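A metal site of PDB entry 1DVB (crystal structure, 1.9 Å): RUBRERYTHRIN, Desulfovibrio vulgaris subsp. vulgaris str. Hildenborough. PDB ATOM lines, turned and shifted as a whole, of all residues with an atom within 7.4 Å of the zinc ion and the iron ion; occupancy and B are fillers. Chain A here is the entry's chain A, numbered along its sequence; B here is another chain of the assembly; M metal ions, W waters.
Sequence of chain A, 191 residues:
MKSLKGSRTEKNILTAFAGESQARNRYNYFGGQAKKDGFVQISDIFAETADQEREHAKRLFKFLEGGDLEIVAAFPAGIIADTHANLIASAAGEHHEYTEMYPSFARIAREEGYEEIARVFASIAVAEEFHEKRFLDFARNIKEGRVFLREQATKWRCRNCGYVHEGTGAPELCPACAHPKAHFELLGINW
The side-chain hydroxyl (OH) of Tyr 27 lies close to the side-chain carboxylate (OE2) of Glu 94, 2.5 Å away. OH of Tyr 102 lies close to OE2 of Glu 20 (3.1 Å). NE2 of His 131 sits at hydrogen-bond distance from OE1 of Gln 52, at 3.2 Å. A ring nitrogen (NE2) of His 56 is in hydrogen-bond range of the backbone carbonyl oxygen (O) of Cys 161 of chain B.
Four residues have an atom within 4 Å of the zinc ion: Glu 20, Glu 53, His 56 and Glu 128.
Four residues have an atom within 4 Å of the iron ion: Glu 53, Glu 94, Glu 128 and His 131. The nearest printed residue that does not touch the iron ion is Tyr 27 (4.3 Å).
The zinc ion is bound by OE2 of Glu 128 (2.1 Å), OE2 of Glu 20 (2.1 Å), OE1 of Glu 53 (2.1 Å) and ND1 of His 56 (2.2 Å). The zinc ion has four donor atoms within binding distance. Slightly farther from the zinc ion lies OE1 of Glu 128 (2.8 Å). Slightly farther from the zinc ion lies the side-chain carboxylate (OE1) of Glu 20 (2.8 Å).
The iron ion is bound by the side-chain carboxylate (OE1) of Glu 128 (2.0 Å), the side-chain carboxylate (OE2) of Glu 94 (2.0 Å), the side-chain carboxylate (OE1) of Glu 94 (2.1 Å), the side-chain carboxylate (OE2) of Glu 53 (2.1 Å), a ring nitrogen (ND1) of His 131 (2.2 Å) and water W1 (2.2 Å).
Water W1 lies within hydrogen-bond range of the side-chain carboxylate of Glu 97 (3.0 Å) and the side-chain carboxylate of Glu 20 (3.3 Å).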
ATOM      1  N   ALA A  16      12.642  -4.397   0.217  1.00  0.00           N
ATOM      2  CA  ALA A  16      13.847  -3.734   0.730  1.00  0.00           C
ATOM      3  C   ALA A  16      15.078  -4.208  -0.060  1.00  0.00           C
ATOM      4  O   ALA A  16      15.870  -3.414  -0.613  1.00  0.00           O
ATOM      5  CB  ALA A  16      13.881  -4.000   2.216  1.00  0.00           C
ATOM      6  N   GLU A  20      17.377  -1.743  -1.963  1.00  0.00           N
ATOM      7  CA  GLU A  20      18.837  -1.681  -1.689  1.00  0.00           C
ATOM      8  C   GLU A  20      19.716  -2.093  -2.901  1.00  0.00           C
ATOM      9  O   GLU A  20      20.813  -1.557  -3.154  1.00  0.00           O
ATOM     10  CB  GLU A  20      19.167  -2.538  -0.488  1.00  0.00           C
ATOM     11  CG  GLU A  20      18.571  -2.272   0.861  1.00  0.00           C
ATOM     12  CD  GLU A  20      19.055  -1.113   1.727  1.00  0.00           C
ATOM     13  OE1 GLU A  20      18.892   0.091   1.382  1.00  0.00           O
ATOM     14  OE2 GLU A  20      19.636  -1.334   2.836  1.00  0.00           O
ATOM     15  N   ALA A  23      20.099   0.600  -5.120  1.00  0.00           N
ATOM     16  CA  ALA A  23      20.834   1.720  -4.516  1.00  0.00           C
ATOM     17  C   ALA A  23      22.321   1.482  -4.695  1.00  0.00           C
ATOM     18  O   ALA A  23      23.072   2.430  -4.933  1.00  0.00           O
ATOM     19  CB  ALA A  23      20.453   1.905  -3.050  1.00  0.00           C
ATOM     20  N   TYR A  27      24.582   4.317  -6.324  1.00  0.00           N
ATOM     21  CA  TYR A  27      25.760   4.911  -5.647  1.00  0.00           C
ATOM     22  C   TYR A  27      27.004   4.638  -6.478  1.00  0.00           C
ATOM     23  O   TYR A  27      27.870   5.509  -6.632  1.00  0.00           O
ATOM     24  CB  TYR A  27      25.944   4.381  -4.244  1.00  0.00           C
ATOM     25  CG  TYR A  27      24.767   4.753  -3.325  1.00  0.00           C
ATOM     26  CD1 TYR A  27      23.989   5.892  -3.594  1.00  0.00           C
ATOM     27  CD2 TYR A  27      24.452   3.986  -2.224  1.00  0.00           C
ATOM     28  CE1 TYR A  27      22.926   6.220  -2.765  1.00  0.00           C
ATOM     29  CE2 TYR A  27      23.376   4.291  -1.362  1.00  0.00           C
ATOM     30  CZ  TYR A  27      22.640   5.425  -1.665  1.00  0.00           C
ATOM     31  OH  TYR A  27      21.586   5.738  -0.822  1.00  0.00           O
ATOM     32  N   THR A  49      29.675   3.380   0.224  1.00  0.00           N
ATOM     33  CA  THR A  49      28.249   3.225   0.534  1.00  0.00           C
ATOM     34  C   THR A  49      27.635   2.130  -0.326  1.00  0.00           C
ATOM     35  O   THR A  49      26.882   1.278   0.224  1.00  0.00           O
ATOM     36  CB  THR A  49      27.529   4.568   0.367  1.00  0.00           C
ATOM     37  OG1 THR A  49      28.226   5.576   1.146  1.00  0.00           O
ATOM     38  CG2 THR A  49      26.122   4.500   0.932  1.00  0.00           C
ATOM     39  N   GLN A  52      28.437  -1.095   1.203  1.00  0.00           N
ATOM     40  CA  GLN A  52      27.631  -1.364   2.425  1.00  0.00           C
ATOM     41  C   GLN A  52      26.193  -1.695   2.039  1.00  0.00           C
ATOM     42  O   GLN A  52      25.575  -2.493   2.720  1.00  0.00           O
ATOM     43  CB  GLN A  52      27.752  -0.180   3.376  1.00  0.00           C
ATOM     44  CG  GLN A  52      29.212  -0.164   3.889  1.00  0.00           C
ATOM     45  CD  GLN A  52      29.564   1.013   4.814  1.00  0.00           C
ATOM     46  OE1 GLN A  52      28.927   2.085   4.752  1.00  0.00           O
ATOM     47  NE2 GLN A  52      30.566   0.794   5.658  1.00  0.00           N
ATOM     48  N   GLU A  53      25.654  -1.109   0.973  1.00  0.00           N
ATOM     49  CA  GLU A  53      24.297  -1.508   0.558  1.00  0.00           C
ATOM     50  C   GLU A  53      24.209  -2.983   0.175  1.00  0.00           C
ATOM     51  O   GLU A  53      23.261  -3.799   0.372  1.00  0.00           O
ATOM     52  CB  GLU A  53      23.904  -0.558  -0.553  1.00  0.00           C
ATOM     53  CG  GLU A  53      23.784   0.928  -0.215  1.00  0.00           C
ATOM     54  CD  GLU A  53      22.868   1.304   0.908  1.00  0.00           C
ATOM     55  OE1 GLU A  53      21.839   0.666   1.199  1.00  0.00           O
ATOM     56  OE2 GLU A  53      23.056   2.290   1.663  1.00  0.00           O
ATOM     57  N   ARG A  54      25.302  -3.448  -0.443  1.00  0.00           N
ATOM     58  CA  ARG A  54      25.347  -4.841  -0.877  1.00  0.00           C
ATOM     59  C   ARG A  54      25.246  -5.751   0.315  1.00  0.00           C
ATOM     60  O   ARG A  54      24.718  -6.849   0.253  1.00  0.00           O
ATOM     61  CB  ARG A  54      26.658  -5.092  -1.633  1.00  0.00           C
ATOM     62  CG  ARG A  54      27.065  -6.567  -1.667  1.00  0.00           C
ATOM     63  CD  ARG A  54      28.524  -6.693  -2.102  1.00  0.00           C
ATOM     64  NE  ARG A  54      29.426  -6.615  -0.949  1.00  0.00           N
ATOM     65  CZ  ARG A  54      30.653  -6.140  -0.960  1.00  0.00           C
ATOM     66  NH1 ARG A  54      31.224  -5.667  -2.036  1.00  0.00           N
ATOM     67  NH2 ARG A  54      31.345  -6.143   0.163  1.00  0.00           N
ATOM     68  N   GLU A  55      25.805  -5.178   1.425  1.00  0.00           N
ATOM     69  CA  GLU A  55      25.846  -6.079   2.588  1.00  0.00           C
ATOM     70  C   GLU A  55      24.570  -6.018   3.402  1.00  0.00           C
ATOM     71  O   GLU A  55      24.171  -6.932   4.098  1.00  0.00           O
ATOM     72  CB  GLU A  55      27.115  -5.730   3.400  1.00  0.00           C
ATOM     73  CG  GLU A  55      28.410  -5.877   2.595  1.00  0.00           C
ATOM     74  CD  GLU A  55      28.684  -7.375   2.404  1.00  0.00           C
ATOM     75  OE1 GLU A  55      28.385  -8.124   3.343  1.00  0.00           O
ATOM     76  OE2 GLU A  55      29.167  -7.774   1.324  1.00  0.00           O
ATOM     77  N   HIS A  56      23.822  -4.925   3.358  1.00  0.00           N
ATOM     78  CA  HIS A  56      22.496  -4.902   3.940  1.00  0.00           C
ATOM     79  C   HIS A  56      21.611  -5.863   3.114  1.00  0.00           C
ATOM     80  O   HIS A  56      20.850  -6.649   3.647  1.00  0.00           O
ATOM     81  CB  HIS A  56      21.840  -3.527   3.906  1.00  0.00           C
ATOM     82  CG  HIS A  56      22.570  -2.480   4.640  1.00  0.00           C
ATOM     83  ND1 HIS A  56      22.444  -1.141   4.379  1.00  0.00           N
ATOM     84  CD2 HIS A  56      23.445  -2.583   5.672  1.00  0.00           C
ATOM     85  CE1 HIS A  56      23.226  -0.463   5.208  1.00  0.00           C
ATOM     86  NE2 HIS A  56      23.844  -1.320   6.009  1.00  0.00           N
ATOM     87  N   ALA A  57      21.729  -5.758   1.785  1.00  0.00           N
ATOM     88  CA  ALA A  57      20.928  -6.644   0.897  1.00  0.00           C
ATOM     89  C   ALA A  57      21.221  -8.093   1.193  1.00  0.00           C
ATOM     90  O   ALA A  57      20.388  -9.001   1.274  1.00  0.00           O
ATOM     91  CB  ALA A  57      21.215  -6.241  -0.551  1.00  0.00           C
ATOM     92  N   SER A  90      20.506  11.265  -3.067  1.00  0.00           N
ATOM     93  CA  SER A  90      20.850  10.103  -2.250  1.00  0.00           C
ATOM     94  C   SER A  90      20.379  10.213  -0.815  1.00  0.00           C
ATOM     95  O   SER A  90      19.878   9.326  -0.093  1.00  0.00           O
ATOM     96  CB  SER A  90      22.373   9.914  -2.325  1.00  0.00           C
ATOM     97  OG  SER A  90      22.788   9.627  -3.662  1.00  0.00           O
ATOM     98  N   GLY A  93      16.755   9.719  -0.237  1.00  0.00           N
ATOM     99  CA  GLY A  93      16.190   8.367  -0.212  1.00  0.00           C
ATOM    100  C   GLY A  93      16.591   7.594   0.997  1.00  0.00           C
ATOM    101  O   GLY A  93      15.879   6.724   1.512  1.00  0.00           O
ATOM    102  N   GLU A  94      17.798   7.980   1.419  1.00  0.00           N
ATOM    103  CA  GLU A  94      18.237   7.442   2.705  1.00  0.00           C
ATOM    104  C   GLU A  94      17.248   7.962   3.729  1.00  0.00           C
ATOM    105  O   GLU A  94      16.781   7.294   4.646  1.00  0.00           O
ATOM    106  CB  GLU A  94      19.683   7.841   2.940  1.00  0.00           C
ATOM    107  CG  GLU A  94      20.691   7.269   1.948  1.00  0.00           C
ATOM    108  CD  GLU A  94      21.214   5.902   2.261  1.00  0.00           C
ATOM    109  OE1 GLU A  94      20.873   5.220   3.274  1.00  0.00           O
ATOM    110  OE2 GLU A  94      22.036   5.214   1.614  1.00  0.00           O
ATOM    111  N   GLU A  97      13.905   6.096   3.757  1.00  0.00           N
ATOM    112  CA  GLU A  97      14.167   4.797   4.333  1.00  0.00           C
ATOM    113  C   GLU A  97      14.291   4.698   5.850  1.00  0.00           C
ATOM    114  O   GLU A  97      13.696   3.758   6.428  1.00  0.00           O
ATOM    115  CB  GLU A  97      15.499   4.328   3.739  1.00  0.00           C
ATOM    116  CG  GLU A  97      15.355   3.789   2.323  1.00  0.00           C
ATOM    117  CD  GLU A  97      16.712   3.593   1.680  1.00  0.00           C
ATOM    118  OE1 GLU A  97      17.649   3.125   2.368  1.00  0.00           O
ATOM    119  OE2 GLU A  97      16.787   3.936   0.488  1.00  0.00           O
ATOM    120  N   TYR A 102      11.883   1.554   6.868  1.00  0.00           N
ATOM    121  CA  TYR A 102      12.274   0.491   7.786  1.00  0.00           C
ATOM    122  C   TYR A 102      11.575   0.566   9.137  1.00  0.00           C
ATOM    123  O   TYR A 102      11.361  -0.550   9.670  1.00  0.00           O
ATOM    124  CB  TYR A 102      13.806   0.493   7.995  1.00  0.00           C
ATOM    125  CG  TYR A 102      14.553  -0.053   6.788  1.00  0.00           C
ATOM    126  CD1 TYR A 102      14.582  -1.409   6.519  1.00  0.00           C
ATOM    127  CD2 TYR A 102      15.220   0.807   5.923  1.00  0.00           C
ATOM    128  CE1 TYR A 102      15.244  -1.943   5.430  1.00  0.00           C
ATOM    129  CE2 TYR A 102      15.893   0.295   4.829  1.00  0.00           C
ATOM    130  CZ  TYR A 102      15.900  -1.062   4.587  1.00  0.00           C
ATOM    131  OH  TYR A 102      16.573  -1.539   3.488  1.00  0.00           O
ATOM    132  N   ILE A 124      19.729  -1.762  10.331  1.00  0.00           N
ATOM    133  CA  ILE A 124      20.001  -1.074   9.060  1.00  0.00           C
ATOM    134  C   ILE A 124      19.577   0.379   9.020  1.00  0.00           C
ATOM    135  O   ILE A 124      20.241   1.268   8.434  1.00  0.00           O
ATOM    136  CB  ILE A 124      19.261  -1.830   7.942  1.00  0.00           C
ATOM    137  CG1 ILE A 124      19.785  -3.260   7.768  1.00  0.00           C
ATOM    138  CG2 ILE A 124      19.295  -1.059   6.631  1.00  0.00           C
ATOM    139  CD1 ILE A 124      18.846  -4.036   6.846  1.00  0.00           C
ATOM    140  N   ALA A 125      18.433   0.739   9.621  1.00  0.00           N
ATOM    141  CA  ALA A 125      17.974   2.134   9.683  1.00  0.00           C
ATOM    142  C   ALA A 125      19.089   3.020  10.265  1.00  0.00           C
ATOM    143  O   ALA A 125      19.311   4.118   9.774  1.00  0.00           O
ATOM    144  CB  ALA A 125      16.708   2.308  10.520  1.00  0.00           C
ATOM    145  N   ALA A 127      22.303   2.603  10.142  1.00  0.00           N
ATOM    146  CA  ALA A 127      23.320   2.807   9.115  1.00  0.00           C
ATOM    147  C   ALA A 127      22.854   3.814   8.097  1.00  0.00           C
ATOM    148  O   ALA A 127      23.622   4.664   7.655  1.00  0.00           O
ATOM    149  CB  ALA A 127      23.669   1.497   8.381  1.00  0.00           C
ATOM    150  N   GLU A 128      21.546   3.672   7.739  1.00  0.00           N
ATOM    151  CA  GLU A 128      21.180   4.645   6.701  1.00  0.00           C
ATOM    152  C   GLU A 128      21.166   6.022   7.349  1.00  0.00           C
ATOM    153  O   GLU A 128      21.337   6.989   6.626  1.00  0.00           O
ATOM    154  CB  GLU A 128      19.868   4.396   5.973  1.00  0.00           C
ATOM    155  CG  GLU A 128      19.525   2.958   5.695  1.00  0.00           C
ATOM    156  CD  GLU A 128      20.354   2.235   4.656  1.00  0.00           C
ATOM    157  OE1 GLU A 128      21.586   2.476   4.451  1.00  0.00           O
ATOM    158  OE2 GLU A 128      19.733   1.346   3.989  1.00  0.00           O
ATOM    159  N   GLU A 129      20.959   6.109   8.680  1.00  0.00           N
ATOM    160  CA  GLU A 129      21.004   7.516   9.120  1.00  0.00           C
ATOM    161  C   GLU A 129      22.408   8.112   8.984  1.00  0.00           C
ATOM    162  O   GLU A 129      22.485   9.295   8.613  1.00  0.00           O
ATOM    163  CB  GLU A 129      20.483   7.661  10.562  1.00  0.00           C
ATOM    164  CG  GLU A 129      20.245   9.158  10.861  1.00  0.00           C
ATOM    165  CD  GLU A 129      19.619   9.444  12.217  1.00  0.00           C
ATOM    166  OE1 GLU A 129      19.308   8.465  12.934  1.00  0.00           O
ATOM    167  OE2 GLU A 129      19.447  10.663  12.534  1.00  0.00           O
ATOM    168  N   PHE A 130      23.501   7.407   9.221  1.00  0.00           N
ATOM    169  CA  PHE A 130      24.855   7.962   9.066  1.00  0.00           C
ATOM    170  C   PHE A 130      25.151   8.225   7.594  1.00  0.00           C
ATOM    171  O   PHE A 130      25.828   9.213   7.214  1.00  0.00           O
ATOM    172  CB  PHE A 130      25.805   7.007   9.804  1.00  0.00           C
ATOM    173  CG  PHE A 130      27.241   7.470   9.560  1.00  0.00           C
ATOM    174  CD1 PHE A 130      27.622   8.772   9.850  1.00  0.00           C
ATOM    175  CD2 PHE A 130      28.215   6.621   9.058  1.00  0.00           C
ATOM    176  CE1 PHE A 130      28.917   9.212   9.620  1.00  0.00           C
ATOM    177  CE2 PHE A 130      29.521   7.041   8.820  1.00  0.00           C
ATOM    178  CZ  PHE A 130      29.882   8.344   9.095  1.00  0.00           C
ATOM    179  N   HIS A 131      24.609   7.321   6.730  1.00  0.00           N
ATOM    180  CA  HIS A 131      24.863   7.546   5.303  1.00  0.00           C
ATOM    181  C   HIS A 131      24.313   8.897   4.910  1.00  0.00           C
ATOM    182  O   HIS A 131      24.921   9.723   4.231  1.00  0.00           O
ATOM    183  CB  HIS A 131      24.262   6.471   4.360  1.00  0.00           C
ATOM    184  CG  HIS A 131      24.726   5.045   4.417  1.00  0.00           C
ATOM    185  ND1 HIS A 131      23.970   3.935   4.067  1.00  0.00           N
ATOM    186  CD2 HIS A 131      25.936   4.555   4.803  1.00  0.00           C
ATOM    187  CE1 HIS A 131      24.731   2.852   4.262  1.00  0.00           C
ATOM    188  NE2 HIS A 131      25.937   3.187   4.702  1.00  0.00           N
ATOM    189  N   GLU A 132      23.087   9.208   5.326  1.00  0.00           N
ATOM    190  CA  GLU A 132      22.516  10.502   4.942  1.00  0.00           C
ATOM    191  C   GLU A 132      23.337  11.687   5.442  1.00  0.00           C
ATOM    192  O   GLU A 132      23.596  12.671   4.759  1.00  0.00           O
ATOM    193  CB  GLU A 132      21.083  10.699   5.476  1.00  0.00           C
ATOM    194  CG  GLU A 132      20.583  12.099   5.096  1.00  0.00           C
ATOM    195  CD  GLU A 132      19.314  12.529   5.831  1.00  0.00           C
ATOM    196  OE1 GLU A 132      19.091  12.106   6.968  1.00  0.00           O
ATOM    197  OE2 GLU A 132      18.515  13.319   5.280  1.00  0.00           O
ATOM    198  N   PHE A 135      26.274  12.273   3.385  1.00  0.00           N
ATOM    199  CA  PHE A 135      25.976  12.854   2.081  1.00  0.00           C
ATOM    200  C   PHE A 135      25.654  14.328   2.211  1.00  0.00           C
ATOM    201  O   PHE A 135      26.079  15.111   1.365  1.00  0.00           O
ATOM    202  CB  PHE A 135      24.806  12.089   1.405  1.00  0.00           C
ATOM    203  CG  PHE A 135      25.270  10.764   0.782  1.00  0.00           C
ATOM    204  CD1 PHE A 135      26.487  10.625   0.150  1.00  0.00           C
ATOM    205  CD2 PHE A 135      24.456   9.638   0.826  1.00  0.00           C
ATOM    206  CE1 PHE A 135      26.920   9.430  -0.415  1.00  0.00           C
ATOM    207  CE2 PHE A 135      24.848   8.456   0.288  1.00  0.00           C
ATOM    208  CZ  PHE A 135      26.075   8.359  -0.340  1.00  0.00           C
ATOM    209  N   CYS B 161      29.093  -2.795   6.961  1.00  0.00           N
ATOM    210  CA  CYS B 161      27.792  -2.277   6.602  1.00  0.00           C
ATOM    211  C   CYS B 161      27.524  -0.867   7.120  1.00  0.00           C
ATOM    212  O   CYS B 161      26.392  -0.479   6.772  1.00  0.00           O
ATOM    213  CB  CYS B 161      26.590  -3.075   7.143  1.00  0.00           C
ATOM    214  SG  CYS B 161      26.403  -3.050   8.925  1.00  0.00           S
HETATM  215 ZN    ZN M   1      21.150   0.097   3.107  1.00  0.00          ZN
HETATM  216 FE    FE M   2      22.145   3.649   2.916  1.00  0.00          FE
HETATM  217  O   HOH W   1      20.553   2.944   1.581  1.00  0.00           O
